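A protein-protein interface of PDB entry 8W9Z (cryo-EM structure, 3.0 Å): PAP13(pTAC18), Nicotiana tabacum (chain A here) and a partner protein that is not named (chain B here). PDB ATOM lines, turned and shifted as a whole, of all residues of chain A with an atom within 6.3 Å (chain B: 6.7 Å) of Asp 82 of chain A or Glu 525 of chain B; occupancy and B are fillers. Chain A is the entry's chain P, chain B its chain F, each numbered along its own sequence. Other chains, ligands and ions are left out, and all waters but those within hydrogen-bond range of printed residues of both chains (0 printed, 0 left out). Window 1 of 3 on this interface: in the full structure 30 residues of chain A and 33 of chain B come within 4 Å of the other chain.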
ATOM      1  N   PRO A  80      14.144 -17.807  -1.077  1.00  0.00           N
ATOM      2  CA  PRO A  80      13.847 -17.132  -2.347  1.00  0.00           C
ATOM      3  C   PRO A  80      12.600 -16.273  -2.201  1.00  0.00           C
ATOM      4  O   PRO A  80      11.532 -16.767  -1.832  1.00  0.00           O
ATOM      5  CB  PRO A  80      13.624 -18.291  -3.327  1.00  0.00           C
ATOM      6  CG  PRO A  80      14.233 -19.489  -2.664  1.00  0.00           C
ATOM      7  CD  PRO A  80      14.046 -19.269  -1.196  1.00  0.00           C
ATOM      8  N   TRP A  81      12.740 -14.981  -2.487  1.00  0.00           N
ATOM      9  CA  TRP A  81      11.640 -14.050  -2.272  1.00  0.00           C
ATOM     10  C   TRP A  81      11.607 -13.019  -3.388  1.00  0.00           C
ATOM     11  O   TRP A  81      12.649 -12.477  -3.769  1.00  0.00           O
ATOM     12  CB  TRP A  81      11.769 -13.354  -0.914  1.00  0.00           C
ATOM     13  CG  TRP A  81      10.490 -12.749  -0.431  1.00  0.00           C
ATOM     14  CD1 TRP A  81      10.048 -11.479  -0.654  1.00  0.00           C
ATOM     15  CD2 TRP A  81       9.482 -13.393   0.355  1.00  0.00           C
ATOM     16  NE1 TRP A  81       8.827 -11.291  -0.055  1.00  0.00           N
ATOM     17  CE2 TRP A  81       8.457 -12.452   0.571  1.00  0.00           C
ATOM     18  CE3 TRP A  81       9.345 -14.675   0.897  1.00  0.00           C
ATOM     19  CZ2 TRP A  81       7.312 -12.751   1.307  1.00  0.00           C
ATOM     20  CZ3 TRP A  81       8.208 -14.970   1.626  1.00  0.00           C
ATOM     21  CH2 TRP A  81       7.207 -14.012   1.825  1.00  0.00           C
ATOM     22  N   ASP A  82      10.410 -12.758  -3.906  1.00  0.00           N
ATOM     23  CA  ASP A  82      10.172 -11.707  -4.884  1.00  0.00           C
ATOM     24  C   ASP A  82       9.425 -10.568  -4.207  1.00  0.00           C
ATOM     25  O   ASP A  82       8.355 -10.782  -3.627  1.00  0.00           O
ATOM     26  CB  ASP A  82       9.371 -12.235  -6.075  1.00  0.00           C
ATOM     27  CG  ASP A  82       8.911 -11.130  -7.004  1.00  0.00           C
ATOM     28  OD1 ASP A  82       9.773 -10.489  -7.642  1.00  0.00           O
ATOM     29  OD2 ASP A  82       7.687 -10.899  -7.095  1.00  0.00           O
ATOM     30  N   TRP A  83       9.987  -9.366  -4.279  1.00  0.00           N
ATOM     31  CA  TRP A  83       9.415  -8.224  -3.580  1.00  0.00           C
ATOM     32  C   TRP A  83       8.274  -7.608  -4.377  1.00  0.00           C
ATOM     33  O   TRP A  83       8.315  -7.542  -5.607  1.00  0.00           O
ATOM     34  CB  TRP A  83      10.488  -7.170  -3.315  1.00  0.00           C
ATOM     35  CG  TRP A  83      11.257  -7.391  -2.053  1.00  0.00           C
ATOM     36  CD1 TRP A  83      11.073  -6.755  -0.863  1.00  0.00           C
ATOM     37  CD2 TRP A  83      12.334  -8.311  -1.855  1.00  0.00           C
ATOM     38  NE1 TRP A  83      11.969  -7.222   0.067  1.00  0.00           N
ATOM     39  CE2 TRP A  83      12.755  -8.178  -0.518  1.00  0.00           C
ATOM     40  CE3 TRP A  83      12.985  -9.236  -2.676  1.00  0.00           C
ATOM     41  CZ2 TRP A  83      13.794  -8.933   0.016  1.00  0.00           C
ATOM     42  CZ3 TRP A  83      14.017  -9.985  -2.145  1.00  0.00           C
ATOM     43  CH2 TRP A  83      14.411  -9.829  -0.812  1.00  0.00           C
ATOM     44  N   HIS A  84       7.246  -7.157  -3.656  1.00  0.00           N
ATOM     45  CA  HIS A  84       6.140  -6.421  -4.248  1.00  0.00           C
ATOM     46  C   HIS A  84       6.056  -4.980  -3.773  1.00  0.00           C
ATOM     47  O   HIS A  84       5.414  -4.166  -4.443  1.00  0.00           O
ATOM     48  CB  HIS A  84       4.805  -7.117  -3.945  1.00  0.00           C
ATOM     49  CG  HIS A  84       4.701  -8.503  -4.497  1.00  0.00           C
ATOM     50  ND1 HIS A  84       4.625  -8.762  -5.849  1.00  0.00           N
ATOM     51  CD2 HIS A  84       4.649  -9.707  -3.880  1.00  0.00           C
ATOM     52  CE1 HIS A  84       4.537 -10.067  -6.041  1.00  0.00           C
ATOM     53  NE2 HIS A  84       4.549 -10.663  -4.863  1.00  0.00           N
ATOM     54  N   VAL A  85       6.678  -4.649  -2.644  1.00  0.00           N
ATOM     55  CA  VAL A  85       6.722  -3.298  -2.108  1.00  0.00           C
ATOM     56  C   VAL A  85       8.101  -3.070  -1.497  1.00  0.00           C
ATOM     57  O   VAL A  85       8.931  -3.978  -1.430  1.00  0.00           O
ATOM     58  CB  VAL A  85       5.618  -3.045  -1.060  1.00  0.00           C
ATOM     59  CG1 VAL A  85       4.266  -2.896  -1.733  1.00  0.00           C
ATOM     60  CG2 VAL A  85       5.589  -4.171  -0.039  1.00  0.00           C
ATOM     61  N   TRP A 120      10.209  -4.990  -7.112  1.00  0.00           N
ATOM     62  CA  TRP A 120      10.479  -5.891  -8.234  1.00  0.00           C
ATOM     63  C   TRP A 120      11.864  -6.526  -8.132  1.00  0.00           C
ATOM     64  O   TRP A 120      12.505  -6.810  -9.146  1.00  0.00           O
ATOM     65  CB  TRP A 120      10.317  -5.169  -9.575  1.00  0.00           C
ATOM     66  CG  TRP A 120       8.973  -4.539  -9.749  1.00  0.00           C
ATOM     67  CD1 TRP A 120       7.768  -5.077  -9.410  1.00  0.00           C
ATOM     68  CD2 TRP A 120       8.697  -3.241 -10.289  1.00  0.00           C
ATOM     69  NE1 TRP A 120       6.757  -4.200  -9.715  1.00  0.00           N
ATOM     70  CE2 TRP A 120       7.302  -3.064 -10.253  1.00  0.00           C
ATOM     71  CE3 TRP A 120       9.494  -2.214 -10.801  1.00  0.00           C
ATOM     72  CZ2 TRP A 120       6.686  -1.903 -10.711  1.00  0.00           C
ATOM     73  CZ3 TRP A 120       8.881  -1.063 -11.254  1.00  0.00           C
ATOM     74  CH2 TRP A 120       7.491  -0.917 -11.206  1.00  0.00           C
ATOM     75  N   PHE A 121      12.331  -6.751  -6.908  1.00  0.00           N
ATOM     76  CA  PHE A 121      13.631  -7.359  -6.667  1.00  0.00           C
ATOM     77  C   PHE A 121      13.466  -8.865  -6.505  1.00  0.00           C
ATOM     78  O   PHE A 121      12.603  -9.324  -5.750  1.00  0.00           O
ATOM     79  CB  PHE A 121      14.274  -6.751  -5.419  1.00  0.00           C
ATOM     80  CG  PHE A 121      15.745  -7.040  -5.276  1.00  0.00           C
ATOM     81  CD1 PHE A 121      16.467  -7.606  -6.311  1.00  0.00           C
ATOM     82  CD2 PHE A 121      16.401  -6.743  -4.095  1.00  0.00           C
ATOM     83  CE1 PHE A 121      17.815  -7.869  -6.170  1.00  0.00           C
ATOM     84  CE2 PHE A 121      17.748  -7.003  -3.949  1.00  0.00           C
ATOM     85  CZ  PHE A 121      18.455  -7.567  -4.986  1.00  0.00           C
ATOM     86  N   GLU A 122      14.287  -9.628  -7.222  1.00  0.00           N
ATOM     87  CA  GLU A 122      14.315 -11.081  -7.120  1.00  0.00           C
ATOM     88  C   GLU A 122      15.704 -11.501  -6.663  1.00  0.00           C
ATOM     89  O   GLU A 122      16.689 -11.265  -7.371  1.00  0.00           O
ATOM     90  CB  GLU A 122      13.965 -11.736  -8.458  1.00  0.00           C
ATOM     91  CG  GLU A 122      12.591 -11.369  -8.986  1.00  0.00           C
ATOM     92  CD  GLU A 122      12.273 -12.050 -10.303  1.00  0.00           C
ATOM     93  OE1 GLU A 122      13.131 -12.804 -10.806  1.00  0.00           O
ATOM     94  OE2 GLU A 122      11.163 -11.832 -10.833  1.00  0.00           O
ATOM     95  N   ALA A 123      15.785 -12.115  -5.485  1.00  0.00           N
ATOM     96  CA  ALA A 123      17.069 -12.482  -4.905  1.00  0.00           C
ATOM     97  C   ALA A 123      16.909 -13.766  -4.102  1.00  0.00           C
ATOM     98  O   ALA A 123      15.815 -14.327  -3.992  1.00  0.00           O
ATOM     99  CB  ALA A 123      17.620 -11.348  -4.038  1.00  0.00           C
ATOM    100  N   PHE A 137       7.206  -2.731   5.733  1.00  0.00           N
ATOM    101  CA  PHE A 137       6.961  -2.537   4.312  1.00  0.00           C
ATOM    102  C   PHE A 137       6.272  -1.199   4.076  1.00  0.00           C
ATOM    103  O   PHE A 137       5.217  -0.921   4.653  1.00  0.00           O
ATOM    104  CB  PHE A 137       6.109  -3.677   3.758  1.00  0.00           C
ATOM    105  CG  PHE A 137       6.773  -5.022   3.829  1.00  0.00           C
ATOM    106  CD1 PHE A 137       7.570  -5.471   2.790  1.00  0.00           C
ATOM    107  CD2 PHE A 137       6.597  -5.840   4.931  1.00  0.00           C
ATOM    108  CE1 PHE A 137       8.181  -6.708   2.850  1.00  0.00           C
ATOM    109  CE2 PHE A 137       7.205  -7.078   4.996  1.00  0.00           C
ATOM    110  CZ  PHE A 137       7.999  -7.511   3.954  1.00  0.00           C
ATOM    111  N   ARG B 520       2.707 -13.528   9.513  1.00  0.00           N
ATOM    112  CA  ARG B 520       2.526 -12.112   9.819  1.00  0.00           C
ATOM    113  C   ARG B 520       3.352 -11.239   8.884  1.00  0.00           C
ATOM    114  O   ARG B 520       2.901 -10.164   8.468  1.00  0.00           O
ATOM    115  CB  ARG B 520       2.888 -11.838  11.278  1.00  0.00           C
ATOM    116  CG  ARG B 520       2.624 -10.411  11.725  1.00  0.00           C
ATOM    117  CD  ARG B 520       2.708 -10.281  13.235  1.00  0.00           C
ATOM    118  NE  ARG B 520       4.004 -10.707  13.752  1.00  0.00           N
ATOM    119  CZ  ARG B 520       4.327 -10.718  15.041  1.00  0.00           C
ATOM    120  NH1 ARG B 520       5.530 -11.123  15.423  1.00  0.00           N
ATOM    121  NH2 ARG B 520       3.446 -10.324  15.950  1.00  0.00           N
ATOM    122  N   ARG B 521       4.560 -11.687   8.534  1.00  0.00           N
ATOM    123  CA  ARG B 521       5.366 -10.962   7.556  1.00  0.00           C
ATOM    124  C   ARG B 521       4.659 -10.890   6.207  1.00  0.00           C
ATOM    125  O   ARG B 521       4.591  -9.825   5.582  1.00  0.00           O
ATOM    126  CB  ARG B 521       6.735 -11.627   7.415  1.00  0.00           C
ATOM    127  CG  ARG B 521       7.647 -10.973   6.392  1.00  0.00           C
ATOM    128  CD  ARG B 521       9.016 -11.628   6.390  1.00  0.00           C
ATOM    129  NE  ARG B 521       9.904 -11.051   5.386  1.00  0.00           N
ATOM    130  CZ  ARG B 521      10.089 -11.558   4.173  1.00  0.00           C
ATOM    131  NH1 ARG B 521      10.919 -10.967   3.326  1.00  0.00           N
ATOM    132  NH2 ARG B 521       9.447 -12.658   3.808  1.00  0.00           N
ATOM    133  N   SER B 522       4.124 -12.023   5.743  1.00  0.00           N
ATOM    134  CA  SER B 522       3.404 -12.031   4.472  1.00  0.00           C
ATOM    135  C   SER B 522       2.157 -11.153   4.533  1.00  0.00           C
ATOM    136  O   SER B 522       1.824 -10.457   3.563  1.00  0.00           O
ATOM    137  CB  SER B 522       3.033 -13.461   4.086  1.00  0.00           C
ATOM    138  OG  SER B 522       2.309 -13.487   2.869  1.00  0.00           O
ATOM    139  N   LEU B 523       1.454 -11.174   5.668  1.00  0.00           N
ATOM    140  CA  LEU B 523       0.269 -10.339   5.827  1.00  0.00           C
ATOM    141  C   LEU B 523       0.626  -8.861   5.767  1.00  0.00           C
ATOM    142  O   LEU B 523      -0.076  -8.072   5.127  1.00  0.00           O
ATOM    143  CB  LEU B 523      -0.430 -10.663   7.146  1.00  0.00           C
ATOM    144  CG  LEU B 523      -1.617  -9.763   7.502  1.00  0.00           C
ATOM    145  CD1 LEU B 523      -2.772  -9.987   6.539  1.00  0.00           C
ATOM    146  CD2 LEU B 523      -2.057  -9.982   8.941  1.00  0.00           C
ATOM    147  N   GLU B 524       1.716  -8.467   6.429  1.00  0.00           N
ATOM    148  CA  GLU B 524       2.147  -7.074   6.373  1.00  0.00           C
ATOM    149  C   GLU B 524       2.558  -6.688   4.957  1.00  0.00           C
ATOM    150  O   GLU B 524       2.259  -5.579   4.494  1.00  0.00           O
ATOM    151  CB  GLU B 524       3.295  -6.842   7.354  1.00  0.00           C
ATOM    152  CG  GLU B 524       3.783  -5.405   7.411  1.00  0.00           C
ATOM    153  CD  GLU B 524       4.848  -5.194   8.467  1.00  0.00           C
ATOM    154  OE1 GLU B 524       5.085  -6.122   9.267  1.00  0.00           O
ATOM    155  OE2 GLU B 524       5.448  -4.099   8.498  1.00  0.00           O
ATOM    156  N   GLU B 525       3.233  -7.598   4.250  1.00  0.00           N
ATOM    157  CA  GLU B 525       3.619  -7.324   2.869  1.00  0.00           C
ATOM    158  C   GLU B 525       2.396  -7.068   1.996  1.00  0.00           C
ATOM    159  O   GLU B 525       2.359  -6.100   1.228  1.00  0.00           O
ATOM    160  CB  GLU B 525       4.439  -8.483   2.308  1.00  0.00           C
ATOM    161  CG  GLU B 525       4.830  -8.296   0.852  1.00  0.00           C
ATOM    162  CD  GLU B 525       5.369  -9.564   0.227  1.00  0.00           C
ATOM    163  OE1 GLU B 525       5.088 -10.655   0.764  1.00  0.00           O
ATOM    164  OE2 GLU B 525       6.071  -9.470  -0.802  1.00  0.00           O
ATOM    165  N   ARG B 526       1.380  -7.927   2.100  1.00  0.00           N
ATOM    166  CA  ARG B 526       0.198  -7.731   1.262  1.00  0.00           C
ATOM    167  C   ARG B 526      -0.625  -6.530   1.710  1.00  0.00           C
ATOM    168  O   ARG B 526      -1.259  -5.871   0.877  1.00  0.00           O
ATOM    169  CB  ARG B 526      -0.659  -8.995   1.235  1.00  0.00           C
ATOM    170  CG  ARG B 526      -0.392  -9.857   0.013  1.00  0.00           C
ATOM    171  CD  ARG B 526      -1.309 -11.060  -0.051  1.00  0.00           C
ATOM    172  NE  ARG B 526      -0.948 -11.945  -1.154  1.00  0.00           N
ATOM    173  CZ  ARG B 526       0.002 -12.869  -1.086  1.00  0.00           C
ATOM    174  NH1 ARG B 526       0.693 -13.031   0.035  1.00  0.00           N
ATOM    175  NH2 ARG B 526       0.268 -13.632  -2.136  1.00  0.00           N
ATOM    176  N   GLU B 527      -0.618  -6.214   3.007  1.00  0.00           N
ATOM    177  CA  GLU B 527      -1.291  -5.007   3.471  1.00  0.00           C
ATOM    178  C   GLU B 527      -0.624  -3.757   2.917  1.00  0.00           C
ATOM    179  O   GLU B 527      -1.304  -2.769   2.617  1.00  0.00           O
ATOM    180  CB  GLU B 527      -1.313  -4.979   5.001  1.00  0.00           C
ATOM    181  CG  GLU B 527      -2.032  -3.784   5.608  1.00  0.00           C
ATOM    182  CD  GLU B 527      -1.099  -2.624   5.899  1.00  0.00           C
ATOM    183  OE1 GLU B 527       0.130  -2.800   5.770  1.00  0.00           O
ATOM    184  OE2 GLU B 527      -1.595  -1.534   6.256  1.00  0.00           O
ATOM    185  N   ALA B 528       0.703  -3.781   2.771  1.00  0.00           N
ATOM    186  CA  ALA B 528       1.389  -2.662   2.135  1.00  0.00           C
ATOM    187  C   ALA B 528       1.136  -2.643   0.632  1.00  0.00           C
ATOM    188  O   ALA B 528       1.028  -1.570   0.028  1.00  0.00           O
ATOM    189  CB  ALA B 528       2.887  -2.728   2.425  1.00  0.00           C
ATOM    190  N   MET B 529       1.039  -3.822   0.013  1.00  0.00           N
ATOM    191  CA  MET B 529       0.785  -3.893  -1.424  1.00  0.00           C
ATOM    192  C   MET B 529      -0.593  -3.345  -1.773  1.00  0.00           C
ATOM    193  O   MET B 529      -0.770  -2.713  -2.823  1.00  0.00           O
ATOM    194  CB  MET B 529       0.922  -5.336  -1.907  1.00  0.00           C
ATOM    195  CG  MET B 529       0.757  -5.512  -3.406  1.00  0.00           C
ATOM    196  SD  MET B 529       0.282  -7.190  -3.863  1.00  0.00           S
ATOM    197  CE  MET B 529       1.481  -8.150  -2.942  1.00  0.00           C
ATOM    198  N   LEU B 530      -1.583  -3.588  -0.912  1.00  0.00           N
ATOM    199  CA  LEU B 530      -2.932  -3.101  -1.184  1.00  0.00           C
ATOM    200  C   LEU B 530      -2.988  -1.579  -1.202  1.00  0.00           C
ATOM    201  O   LEU B 530      -3.810  -0.997  -1.920  1.00  0.00           O
ATOM    202  CB  LEU B 530      -3.916  -3.658  -0.154  1.00  0.00           C
ATOM    203  CG  LEU B 530      -4.205  -5.158  -0.238  1.00  0.00           C
ATOM    204  CD1 LEU B 530      -5.218  -5.570   0.819  1.00  0.00           C
ATOM    205  CD2 LEU B 530      -4.691  -5.535  -1.628  1.00  0.00           C
ATOM    206  N   GLU B 544       3.568  -2.882 -12.715  1.00  0.00           N
ATOM    207  CA  GLU B 544       4.544  -3.910 -13.035  1.00  0.00           C
ATOM    208  C   GLU B 544       5.707  -3.275 -13.785  1.00  0.00           C
ATOM    209  O   GLU B 544       5.543  -2.262 -14.471  1.00  0.00           O
ATOM    210  CB  GLU B 544       3.915  -5.029 -13.874  1.00  0.00           C
ATOM    211  CG  GLU B 544       4.786  -6.265 -14.029  1.00  0.00           C
ATOM    212  CD  GLU B 544       5.008  -6.995 -12.718  1.00  0.00           C
ATOM    213  OE1 GLU B 544       4.157  -6.873 -11.812  1.00  0.00           O
ATOM    214  OE2 GLU B 544       6.038  -7.692 -12.592  1.00  0.00           O
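OE2 of Glu 525 of chain B touches O of Asp 82 of chain A, 3.9 Å away. His 84 of chain A touches Glu 525 of chain B. His 84 of chain A touches Met 529 of chain B. CG1 of Val 85 of chain A touches O of Ala 528 of chain B, at 3.9 Å. Val 85 of chain A touches Met 529 of chain B (CG1 to CA, 3.6 Å). Trp 120 of chain A touches Glu 544 of chain B (CZ2 to C, 3.5 Å). O of Arg 521 of chain B touches CE2 of Phe 137 of chain A (3.8 Å). Phe 137 of chain A touches Glu 524 of chain B. Glu 525 of chain B touches Phe 137 of chain A (N to CD2, 3.9 Å). Ala 528 of chain B touches Phe 137 of chain A (CB to CB, 3.6 Å).
N of Trp 81 of chain A lies within hydrogen-bond range of O of Ala 123 of chain A (3.5 Å).
The indole nitrogen (NE1) of Trp 81 of chain A is in hydrogen-bond range of the side-chain carboxylate (OE2) of Glu 525 of chain B (3.4 Å).
Printed residues of chain B within 4 Å of Trp 81 of chain A: Arg 521 (3.3 Å) and Glu 525 (3.1 Å). Of chain B, only Glu 525 (3.9 Å) comes within 4 Å of Asp 82 of chain A. Glu 122 of chain A touches none of the printed residues of chain B. Printed residues of chain B within 4 Å of Phe 137 of chain A: Arg 521, Glu 524, Glu 525 and Ala 528. Printed residues of chain A within 4 Å of Arg 521 of chain B: Trp 81 (3.3 Å) and Phe 137 (3.8 Å). Of chain A, only Trp 81 (3.1 Å), Asp 82 (3.9 Å), His 84 (3.4 Å), Val 85 (3.97 Å) and Phe 137 (3.9 Å) come within 4 Å of Glu 525 of chain B. Of the printed residues of chain A, Met 529 of chain B touches His 84 and Val 85. The nearest residue of chain B that does not touch Asp 82 of chain A is Glu 544 of chain B (6.6 Å). The nearest printed residue of chain B that does not touch Trp 120 of chain A is Glu 525 of chain B (8.8 Å).
Hydrophobic or aromatic side chains of chain B that line the printed part of chain A: Ala 528 and Met 529. Along chain B the printed residues that touch a printed residue of chain A span positions 521 to 544. Hydrophobic or aromatic side chains of chain A within 4 Å of the printed part of chain B: Trp 81, His 84, Val 85, Trp 120 and Phe 137. Among the printed residues, 13 pairs touch across the chains. Among the printed residues, no Asp or Glu carboxylate lies within 4 Å of a Lys or Arg side-chain nitrogen of the other chain.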
